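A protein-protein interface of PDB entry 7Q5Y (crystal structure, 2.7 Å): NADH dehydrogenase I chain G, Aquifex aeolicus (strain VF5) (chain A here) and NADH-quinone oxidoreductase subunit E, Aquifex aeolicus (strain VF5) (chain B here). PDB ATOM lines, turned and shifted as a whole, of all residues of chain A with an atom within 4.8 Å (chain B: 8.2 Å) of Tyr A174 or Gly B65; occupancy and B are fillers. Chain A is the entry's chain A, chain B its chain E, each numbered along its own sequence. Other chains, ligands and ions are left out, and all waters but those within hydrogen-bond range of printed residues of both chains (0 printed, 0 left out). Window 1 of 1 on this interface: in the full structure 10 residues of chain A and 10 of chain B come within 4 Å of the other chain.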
ATOM      1  N   ALA A 172      28.392   1.549  -0.366  1.00  0.00           N
ATOM      2  CA  ALA A 172      27.778   2.871  -0.428  1.00  0.00           C
ATOM      3  C   ALA A 172      27.771   3.523  -1.802  1.00  0.00           C
ATOM      4  O   ALA A 172      27.152   4.578  -1.954  1.00  0.00           O
ATOM      5  CB  ALA A 172      28.503   3.815   0.537  1.00  0.00           C
ATOM      6  N   LEU A 173      28.447   2.956  -2.792  1.00  0.00           N
ATOM      7  CA  LEU A 173      28.476   3.528  -4.124  1.00  0.00           C
ATOM      8  C   LEU A 173      27.861   2.582  -5.131  1.00  0.00           C
ATOM      9  O   LEU A 173      27.853   1.359  -4.954  1.00  0.00           O
ATOM     10  CB  LEU A 173      29.913   3.840  -4.578  1.00  0.00           C
ATOM     11  CG  LEU A 173      30.658   4.783  -3.626  1.00  0.00           C
ATOM     12  CD1 LEU A 173      32.134   4.913  -4.027  1.00  0.00           C
ATOM     13  CD2 LEU A 173      29.962   6.159  -3.606  1.00  0.00           C
ATOM     14  N   TYR A 174      27.381   3.166  -6.217  1.00  0.00           N
ATOM     15  CA  TYR A 174      26.853   2.368  -7.313  1.00  0.00           C
ATOM     16  C   TYR A 174      27.090   3.161  -8.579  1.00  0.00           C
ATOM     17  O   TYR A 174      27.276   4.382  -8.541  1.00  0.00           O
ATOM     18  CB  TYR A 174      25.383   2.000  -7.147  1.00  0.00           C
ATOM     19  CG  TYR A 174      24.413   3.098  -7.460  1.00  0.00           C
ATOM     20  CD1 TYR A 174      23.835   3.208  -8.721  1.00  0.00           C
ATOM     21  CD2 TYR A 174      24.064   4.033  -6.483  1.00  0.00           C
ATOM     22  CE1 TYR A 174      22.941   4.224  -8.997  1.00  0.00           C
ATOM     23  CE2 TYR A 174      23.173   5.034  -6.749  1.00  0.00           C
ATOM     24  CZ  TYR A 174      22.621   5.132  -8.007  1.00  0.00           C
ATOM     25  OH  TYR A 174      21.754   6.147  -8.267  1.00  0.00           O
ATOM     26  N   VAL A 175      27.109   2.460  -9.702  1.00  0.00           N
ATOM     27  CA  VAL A 175      27.329   3.127 -10.974  1.00  0.00           C
ATOM     28  C   VAL A 175      25.970   3.472 -11.541  1.00  0.00           C
ATOM     29  O   VAL A 175      25.157   2.574 -11.791  1.00  0.00           O
ATOM     30  CB  VAL A 175      28.139   2.264 -11.945  1.00  0.00           C
ATOM     31  CG1 VAL A 175      28.216   2.943 -13.280  1.00  0.00           C
ATOM     32  CG2 VAL A 175      29.552   2.093 -11.411  1.00  0.00           C
ATOM     33  N   GLU A 176      25.735   4.774 -11.733  1.00  0.00           N
ATOM     34  CA  GLU A 176      24.490   5.309 -12.262  1.00  0.00           C
ATOM     35  C   GLU A 176      24.636   5.180 -13.762  1.00  0.00           C
ATOM     36  O   GLU A 176      25.743   5.267 -14.299  1.00  0.00           O
ATOM     37  CB  GLU A 176      24.247   6.750 -11.792  1.00  0.00           C
ATOM     38  CG  GLU A 176      22.915   7.441 -12.165  1.00  0.00           C
ATOM     39  CD  GLU A 176      21.665   6.577 -12.042  1.00  0.00           C
ATOM     40  OE1 GLU A 176      21.202   6.303 -10.898  1.00  0.00           O
ATOM     41  OE2 GLU A 176      21.151   6.145 -13.100  1.00  0.00           O
ATOM     42  N   ASN A 183      28.295   7.195 -14.256  1.00  0.00           N
ATOM     43  CA  ASN A 183      28.808   8.069 -13.219  1.00  0.00           C
ATOM     44  C   ASN A 183      28.589   7.471 -11.836  1.00  0.00           C
ATOM     45  O   ASN A 183      27.597   6.795 -11.593  1.00  0.00           O
ATOM     46  CB  ASN A 183      28.138   9.449 -13.317  1.00  0.00           C
ATOM     47  CG  ASN A 183      26.634   9.376 -13.181  1.00  0.00           C
ATOM     48  OD1 ASN A 183      26.109   9.444 -12.073  1.00  0.00           O
ATOM     49  ND2 ASN A 183      25.930   9.254 -14.300  1.00  0.00           N
ATOM     50  N   ILE A 184      29.523   7.731 -10.920  1.00  0.00           N
ATOM     51  CA  ILE A 184      29.430   7.187  -9.561  1.00  0.00           C
ATOM     52  C   ILE A 184      28.441   7.997  -8.714  1.00  0.00           C
ATOM     53  O   ILE A 184      28.450   9.244  -8.714  1.00  0.00           O
ATOM     54  CB  ILE A 184      30.828   7.139  -8.926  1.00  0.00           C
ATOM     55  CG1 ILE A 184      31.823   6.469  -9.894  1.00  0.00           C
ATOM     56  CG2 ILE A 184      30.788   6.497  -7.554  1.00  0.00           C
ATOM     57  CD1 ILE A 184      31.440   5.062 -10.294  1.00  0.00           C
ATOM     58  N   VAL A 185      27.581   7.287  -7.984  1.00  0.00           N
ATOM     59  CA  VAL A 185      26.571   7.921  -7.123  1.00  0.00           C
ATOM     60  C   VAL A 185      26.476   7.216  -5.774  1.00  0.00           C
ATOM     61  O   VAL A 185      26.611   5.974  -5.682  1.00  0.00           O
ATOM     62  CB  VAL A 185      25.178   7.929  -7.784  1.00  0.00           C
ATOM     63  CG1 VAL A 185      24.085   8.459  -6.828  1.00  0.00           C
ATOM     64  CG2 VAL A 185      25.187   8.728  -9.080  1.00  0.00           C
ATOM     65  N   PRO A 186      26.252   7.965  -4.701  1.00  0.00           N
ATOM     66  CA  PRO A 186      26.090   7.335  -3.399  1.00  0.00           C
ATOM     67  C   PRO A 186      24.761   6.600  -3.363  1.00  0.00           C
ATOM     68  O   PRO A 186      23.732   7.096  -3.848  1.00  0.00           O
ATOM     69  CB  PRO A 186      26.105   8.517  -2.423  1.00  0.00           C
ATOM     70  CG  PRO A 186      26.713   9.638  -3.172  1.00  0.00           C
ATOM     71  CD  PRO A 186      26.343   9.429  -4.599  1.00  0.00           C
ATOM     72  N   ALA A 187      24.801   5.400  -2.783  1.00  0.00           N
ATOM     73  CA  ALA A 187      23.614   4.572  -2.688  1.00  0.00           C
ATOM     74  C   ALA A 187      22.514   5.266  -1.920  1.00  0.00           C
ATOM     75  O   ALA A 187      21.333   5.102  -2.238  1.00  0.00           O
ATOM     76  CB  ALA A 187      23.956   3.259  -1.999  1.00  0.00           C
ATOM     77  N   ILE B  30      15.313 -10.084 -10.225  1.00  0.00           N
ATOM     78  CA  ILE B  30      15.393  -8.627 -10.148  1.00  0.00           C
ATOM     79  C   ILE B  30      14.786  -7.934 -11.380  1.00  0.00           C
ATOM     80  O   ILE B  30      14.017  -6.978 -11.241  1.00  0.00           O
ATOM     81  CB  ILE B  30      16.843  -8.194  -9.856  1.00  0.00           C
ATOM     82  CG1 ILE B  30      16.880  -6.718  -9.451  1.00  0.00           C
ATOM     83  CG2 ILE B  30      17.757  -8.477 -11.031  1.00  0.00           C
ATOM     84  CD1 ILE B  30      18.139  -6.346  -8.693  1.00  0.00           C
ATOM     85  N   LEU B  34      11.510  -5.443 -11.299  1.00  0.00           N
ATOM     86  CA  LEU B  34      11.518  -4.051 -11.720  1.00  0.00           C
ATOM     87  C   LEU B  34      10.452  -3.822 -12.777  1.00  0.00           C
ATOM     88  O   LEU B  34       9.835  -2.756 -12.822  1.00  0.00           O
ATOM     89  CB  LEU B  34      12.901  -3.654 -12.219  1.00  0.00           C
ATOM     90  CG  LEU B  34      13.903  -3.677 -11.074  1.00  0.00           C
ATOM     91  CD1 LEU B  34      15.311  -3.559 -11.599  1.00  0.00           C
ATOM     92  CD2 LEU B  34      13.592  -2.612 -10.011  1.00  0.00           C
ATOM     93  N   LEU B  49      13.236   0.757  -4.226  1.00  0.00           N
ATOM     94  CA  LEU B  49      14.448  -0.037  -4.383  1.00  0.00           C
ATOM     95  C   LEU B  49      14.866  -0.690  -3.073  1.00  0.00           C
ATOM     96  O   LEU B  49      15.208  -1.875  -3.064  1.00  0.00           O
ATOM     97  CB  LEU B  49      15.564   0.813  -4.975  1.00  0.00           C
ATOM     98  CG  LEU B  49      15.054   1.418  -6.299  1.00  0.00           C
ATOM     99  CD1 LEU B  49      16.093   2.231  -6.978  1.00  0.00           C
ATOM    100  CD2 LEU B  49      14.555   0.355  -7.244  1.00  0.00           C
ATOM    101  N   PRO B  59      22.135  -6.097  -1.472  1.00  0.00           N
ATOM    102  CA  PRO B  59      22.475  -4.754  -0.998  1.00  0.00           C
ATOM    103  C   PRO B  59      21.833  -3.725  -1.916  1.00  0.00           C
ATOM    104  O   PRO B  59      21.722  -3.925  -3.129  1.00  0.00           O
ATOM    105  CB  PRO B  59      24.007  -4.715  -1.076  1.00  0.00           C
ATOM    106  CG  PRO B  59      24.364  -5.776  -2.007  1.00  0.00           C
ATOM    107  CD  PRO B  59      23.320  -6.851  -1.901  1.00  0.00           C
ATOM    108  N   LEU B  60      21.418  -2.610  -1.314  1.00  0.00           N
ATOM    109  CA  LEU B  60      20.751  -1.554  -2.063  1.00  0.00           C
ATOM    110  C   LEU B  60      21.559  -1.076  -3.263  1.00  0.00           C
ATOM    111  O   LEU B  60      20.994  -0.858  -4.343  1.00  0.00           O
ATOM    112  CB  LEU B  60      20.458  -0.372  -1.151  1.00  0.00           C
ATOM    113  CG  LEU B  60      19.758   0.760  -1.890  1.00  0.00           C
ATOM    114  CD1 LEU B  60      18.448   0.177  -2.409  1.00  0.00           C
ATOM    115  CD2 LEU B  60      19.447   2.001  -0.988  1.00  0.00           C
ATOM    116  N   ASN B  61      22.873  -0.876  -3.091  1.00  0.00           N
ATOM    117  CA  ASN B  61      23.663  -0.378  -4.215  1.00  0.00           C
ATOM    118  C   ASN B  61      23.647  -1.345  -5.393  1.00  0.00           C
ATOM    119  O   ASN B  61      23.763  -0.912  -6.543  1.00  0.00           O
ATOM    120  CB  ASN B  61      25.085  -0.044  -3.777  1.00  0.00           C
ATOM    121  CG  ASN B  61      25.913  -1.272  -3.487  1.00  0.00           C
ATOM    122  OD1 ASN B  61      25.377  -2.316  -3.134  1.00  0.00           O
ATOM    123  ND2 ASN B  61      27.230  -1.139  -3.588  1.00  0.00           N
ATOM    124  N   HIS B  62      23.469  -2.641  -5.135  1.00  0.00           N
ATOM    125  CA  HIS B  62      23.398  -3.618  -6.215  1.00  0.00           C
ATOM    126  C   HIS B  62      22.124  -3.420  -7.027  1.00  0.00           C
ATOM    127  O   HIS B  62      22.163  -3.331  -8.263  1.00  0.00           O
ATOM    128  CB  HIS B  62      23.456  -5.017  -5.636  1.00  0.00           C
ATOM    129  CG  HIS B  62      23.264  -6.089  -6.656  1.00  0.00           C
ATOM    130  ND1 HIS B  62      24.182  -7.085  -6.864  1.00  0.00           N
ATOM    131  CD2 HIS B  62      22.240  -6.341  -7.498  1.00  0.00           C
ATOM    132  CE1 HIS B  62      23.753  -7.878  -7.828  1.00  0.00           C
ATOM    133  NE2 HIS B  62      22.576  -7.449  -8.230  1.00  0.00           N
ATOM    134  N   VAL B  63      20.986  -3.345  -6.338  1.00  0.00           N
ATOM    135  CA  VAL B  63      19.716  -3.096  -7.007  1.00  0.00           C
ATOM    136  C   VAL B  63      19.749  -1.770  -7.746  1.00  0.00           C
ATOM    137  O   VAL B  63      19.264  -1.661  -8.882  1.00  0.00           O
ATOM    138  CB  VAL B  63      18.573  -3.141  -5.992  1.00  0.00           C
ATOM    139  CG1 VAL B  63      17.331  -2.639  -6.633  1.00  0.00           C
ATOM    140  CG2 VAL B  63      18.385  -4.586  -5.526  1.00  0.00           C
ATOM    141  N   GLU B  64      20.312  -0.735  -7.116  1.00  0.00           N
ATOM    142  CA  GLU B  64      20.382   0.565  -7.778  1.00  0.00           C
ATOM    143  C   GLU B  64      21.203   0.469  -9.051  1.00  0.00           C
ATOM    144  O   GLU B  64      20.810   0.993 -10.100  1.00  0.00           O
ATOM    145  CB  GLU B  64      20.962   1.631  -6.847  1.00  0.00           C
ATOM    146  CG  GLU B  64      19.986   2.071  -5.787  1.00  0.00           C
ATOM    147  CD  GLU B  64      20.584   3.068  -4.824  1.00  0.00           C
ATOM    148  OE1 GLU B  64      21.688   2.810  -4.299  1.00  0.00           O
ATOM    149  OE2 GLU B  64      19.942   4.112  -4.604  1.00  0.00           O
ATOM    150  N   GLY B  65      22.355  -0.204  -8.977  1.00  0.00           N
ATOM    151  CA  GLY B  65      23.171  -0.345 -10.166  1.00  0.00           C
ATOM    152  C   GLY B  65      22.447  -1.065 -11.297  1.00  0.00           C
ATOM    153  O   GLY B  65      22.599  -0.708 -12.467  1.00  0.00           O
ATOM    154  N   VAL B  66      21.637  -2.079 -10.964  1.00  0.00           N
ATOM    155  CA  VAL B  66      20.929  -2.815 -11.996  1.00  0.00           C
ATOM    156  C   VAL B  66      19.868  -1.944 -12.653  1.00  0.00           C
ATOM    157  O   VAL B  66      19.840  -1.797 -13.878  1.00  0.00           O
ATOM    158  CB  VAL B  66      20.330  -4.113 -11.431  1.00  0.00           C
ATOM    159  CG1 VAL B  66      19.200  -4.591 -12.335  1.00  0.00           C
ATOM    160  CG2 VAL B  66      21.395  -5.213 -11.323  1.00  0.00           C
ATOM    161  N   VAL B  67      18.979  -1.351 -11.868  1.00  0.00           N
ATOM    162  CA  VAL B  67      17.936  -0.535 -12.475  1.00  0.00           C
ATOM    163  C   VAL B  67      18.510   0.616 -13.285  1.00  0.00           C
ATOM    164  O   VAL B  67      17.865   1.101 -14.219  1.00  0.00           O
ATOM    165  CB  VAL B  67      16.967  -0.044 -11.374  1.00  0.00           C
ATOM    166  CG1 VAL B  67      17.664   0.953 -10.453  1.00  0.00           C
ATOM    167  CG2 VAL B  67      15.684   0.542 -11.985  1.00  0.00           C
ATOM    168  N   ALA B  68      19.723   1.057 -12.971  1.00  0.00           N
ATOM    169  CA  ALA B  68      20.307   2.156 -13.728  1.00  0.00           C
ATOM    170  C   ALA B  68      20.844   1.718 -15.086  1.00  0.00           C
ATOM    171  O   ALA B  68      20.917   2.522 -16.014  1.00  0.00           O
ATOM    172  CB  ALA B  68      21.430   2.798 -12.921  1.00  0.00           C
ATOM    173  N   PHE B  69      21.213   0.460 -15.221  1.00  0.00           N
ATOM    174  CA  PHE B  69      21.813  -0.054 -16.441  1.00  0.00           C
ATOM    175  C   PHE B  69      20.821  -0.316 -17.573  1.00  0.00           C
ATOM    176  O   PHE B  69      21.171  -0.114 -18.726  1.00  0.00           O
ATOM    177  CB  PHE B  69      22.560  -1.341 -16.100  1.00  0.00           C
ATOM    178  CG  PHE B  69      23.247  -1.976 -17.266  1.00  0.00           C
ATOM    179  CD1 PHE B  69      24.576  -1.684 -17.545  1.00  0.00           C
ATOM    180  CD2 PHE B  69      22.582  -2.902 -18.066  1.00  0.00           C
ATOM    181  CE1 PHE B  69      25.233  -2.281 -18.622  1.00  0.00           C
ATOM    182  CE2 PHE B  69      23.227  -3.513 -19.133  1.00  0.00           C
ATOM    183  CZ  PHE B  69      24.558  -3.193 -19.420  1.00  0.00           C
ATOM    184  N   TYR B  70      19.617  -0.803 -17.301  1.00  0.00           N
ATOM    185  CA  TYR B  70      18.684  -1.157 -18.369  1.00  0.00           C
ATOM    186  C   TYR B  70      17.817   0.001 -18.857  1.00  0.00           C
ATOM    187  O   TYR B  70      17.274   0.785 -18.073  1.00  0.00           O
ATOM    188  CB  TYR B  70      17.844  -2.355 -17.927  1.00  0.00           C
ATOM    189  CG  TYR B  70      18.724  -3.560 -17.656  1.00  0.00           C
ATOM    190  CD1 TYR B  70      19.121  -4.414 -18.689  1.00  0.00           C
ATOM    191  CD2 TYR B  70      19.202  -3.820 -16.378  1.00  0.00           C
ATOM    192  CE1 TYR B  70      19.952  -5.521 -18.440  1.00  0.00           C
ATOM    193  CE2 TYR B  70      20.024  -4.913 -16.123  1.00  0.00           C
ATOM    194  CZ  TYR B  70      20.396  -5.754 -17.161  1.00  0.00           C
ATOM    195  OH  TYR B  70      21.216  -6.810 -16.895  1.00  0.00           O
ATOM    196  N   PHE B  73      13.717   0.695 -17.892  1.00  0.00           N
ATOM    197  CA  PHE B  73      13.320   1.219 -16.591  1.00  0.00           C
ATOM    198  C   PHE B  73      13.359   2.754 -16.547  1.00  0.00           C
ATOM    199  O   PHE B  73      14.259   3.392 -17.106  1.00  0.00           O
ATOM    200  CB  PHE B  73      14.222   0.607 -15.536  1.00  0.00           C
ATOM    201  CG  PHE B  73      14.137  -0.872 -15.484  1.00  0.00           C
ATOM    202  CD1 PHE B  73      12.921  -1.511 -15.716  1.00  0.00           C
ATOM    203  CD2 PHE B  73      15.262  -1.640 -15.240  1.00  0.00           C
ATOM    204  CE1 PHE B  73      12.797  -2.903 -15.657  1.00  0.00           C
ATOM    205  CE2 PHE B  73      15.162  -3.046 -15.200  1.00  0.00           C
ATOM    206  CZ  PHE B  73      13.923  -3.668 -15.411  1.00  0.00           C
ATOM    207  N   ARG B  75      12.798   5.856 -13.666  1.00  0.00           N
ATOM    208  CA  ARG B  75      12.591   6.308 -12.298  1.00  0.00           C
ATOM    209  C   ARG B  75      12.225   7.791 -12.210  1.00  0.00           C
ATOM    210  O   ARG B  75      11.941   8.268 -11.115  1.00  0.00           O
ATOM    211  CB  ARG B  75      13.849   6.069 -11.464  1.00  0.00           C
ATOM    212  CG  ARG B  75      14.131   4.639 -11.151  1.00  0.00           C
ATOM    213  CD  ARG B  75      15.560   4.523 -10.705  1.00  0.00           C
ATOM    214  NE  ARG B  75      16.476   4.777 -11.807  1.00  0.00           N
ATOM    215  CZ  ARG B  75      17.769   5.057 -11.663  1.00  0.00           C
ATOM    216  NH1 ARG B  75      18.329   5.151 -10.441  1.00  0.00           N
ATOM    217  NH2 ARG B  75      18.501   5.244 -12.760  1.00  0.00           N
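The backbone carbonyl oxygen (O) of Leu A173 sits at hydrogen-bond distance from the side-chain amide nitrogen (ND2) of Asn B61, at 2.9 Å.
The side-chain carboxylate (OE2) of Glu A176 is in salt-bridge range of the guanidinium group (NH2) of Arg B75, 2.8 Å away.
The backbone carbonyl oxygen of Ala A187 sits close to the side-chain carboxylate of Glu B64 (2.9 Å).
The backbone carbonyl oxygen (O) of Ala A172 is in hydrogen-bond range of the backbone NH (N) of Ala A187 (2.6 Å).
The side-chain carboxylate (OE1) of Glu A176 sits at hydrogen-bond distance from the side-chain hydroxyl (OH) of Tyr A174, at 2.7 Å.
O of Val A185 sits at hydrogen-bond distance from N of Tyr A174 (3.0 Å).
The backbone NH (N) of Glu A176 is in hydrogen-bond range of the backbone carbonyl oxygen (O) of Asn A183 (2.8 Å).
Tyr A174 touches Asn B61 (CB to O, 3.4 Å).
Tyr A174 touches Glu B64.
Gly B65 touches Tyr A174 (N to CD1, 3.7 Å).
Val A175 touches Gly B65.
O of Val A175 touches CB of Ala B68, at 3.9 Å.
CB of Ala B68 touches OE2 of Glu A176 (3.4 Å).
Leu B60 touches Ala A187 (CD2 to O, 3.8 Å).
CB of Ala A187 touches CB of Asn B61, at 3.9 Å.
Of the printed residues of chain B, Leu A173 touches Asn B61 (2.9 Å).
Tyr A174 touches just these residues of chain B: Asn B61 (3.4 Å), Glu B64 (3.5 Å) and Gly B65 (3.7 Å).
Printed residues of chain B within 4 Å of Glu A176: Ala B68 (3.4 Å) and Arg B75 (2.8 Å).
Ile A184 touches none of the printed residues of chain B.
Of the printed residues of chain B, Ala A187 touches Leu B60 (3.8 Å), Asn B61 (3.9 Å) and Glu B64 (2.9 Å).
Of the printed residues of chain A, Asn B61 touches Leu A173, Tyr A174 and Ala A187.
Of the printed residues of chain A, Glu B64 touches Tyr A174 and Ala A187.
Val B67 touches none of the printed residues of chain A.
The nearest residue of chain B that does not touch Tyr A174 is Arg B75 (4.2 Å).
The nearest printed residue of chain A that does not touch Gly B65 is Glu A176 (5.9 Å).
Hydrophobic or aromatic side chains of chain B within 4 Å of the printed part of chain A: Leu B60 and Ala B68.
Of the 10 printed residues of chain A, 5 touch a printed residue of chain B.
Printed residues of chain A that touch a printed residue of chain B: Leu A173, Tyr A174, Val A175, Glu A176 and Ala A187.
Hydrophobic or aromatic side chains of chain A that line the printed part of chain B: Tyr A174 and Ala A187.
Among the printed residues, Asp or Glu carboxylates within 4 Å of a Lys or Arg side-chain nitrogen of the other chain: Glu A176 with Arg B75.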
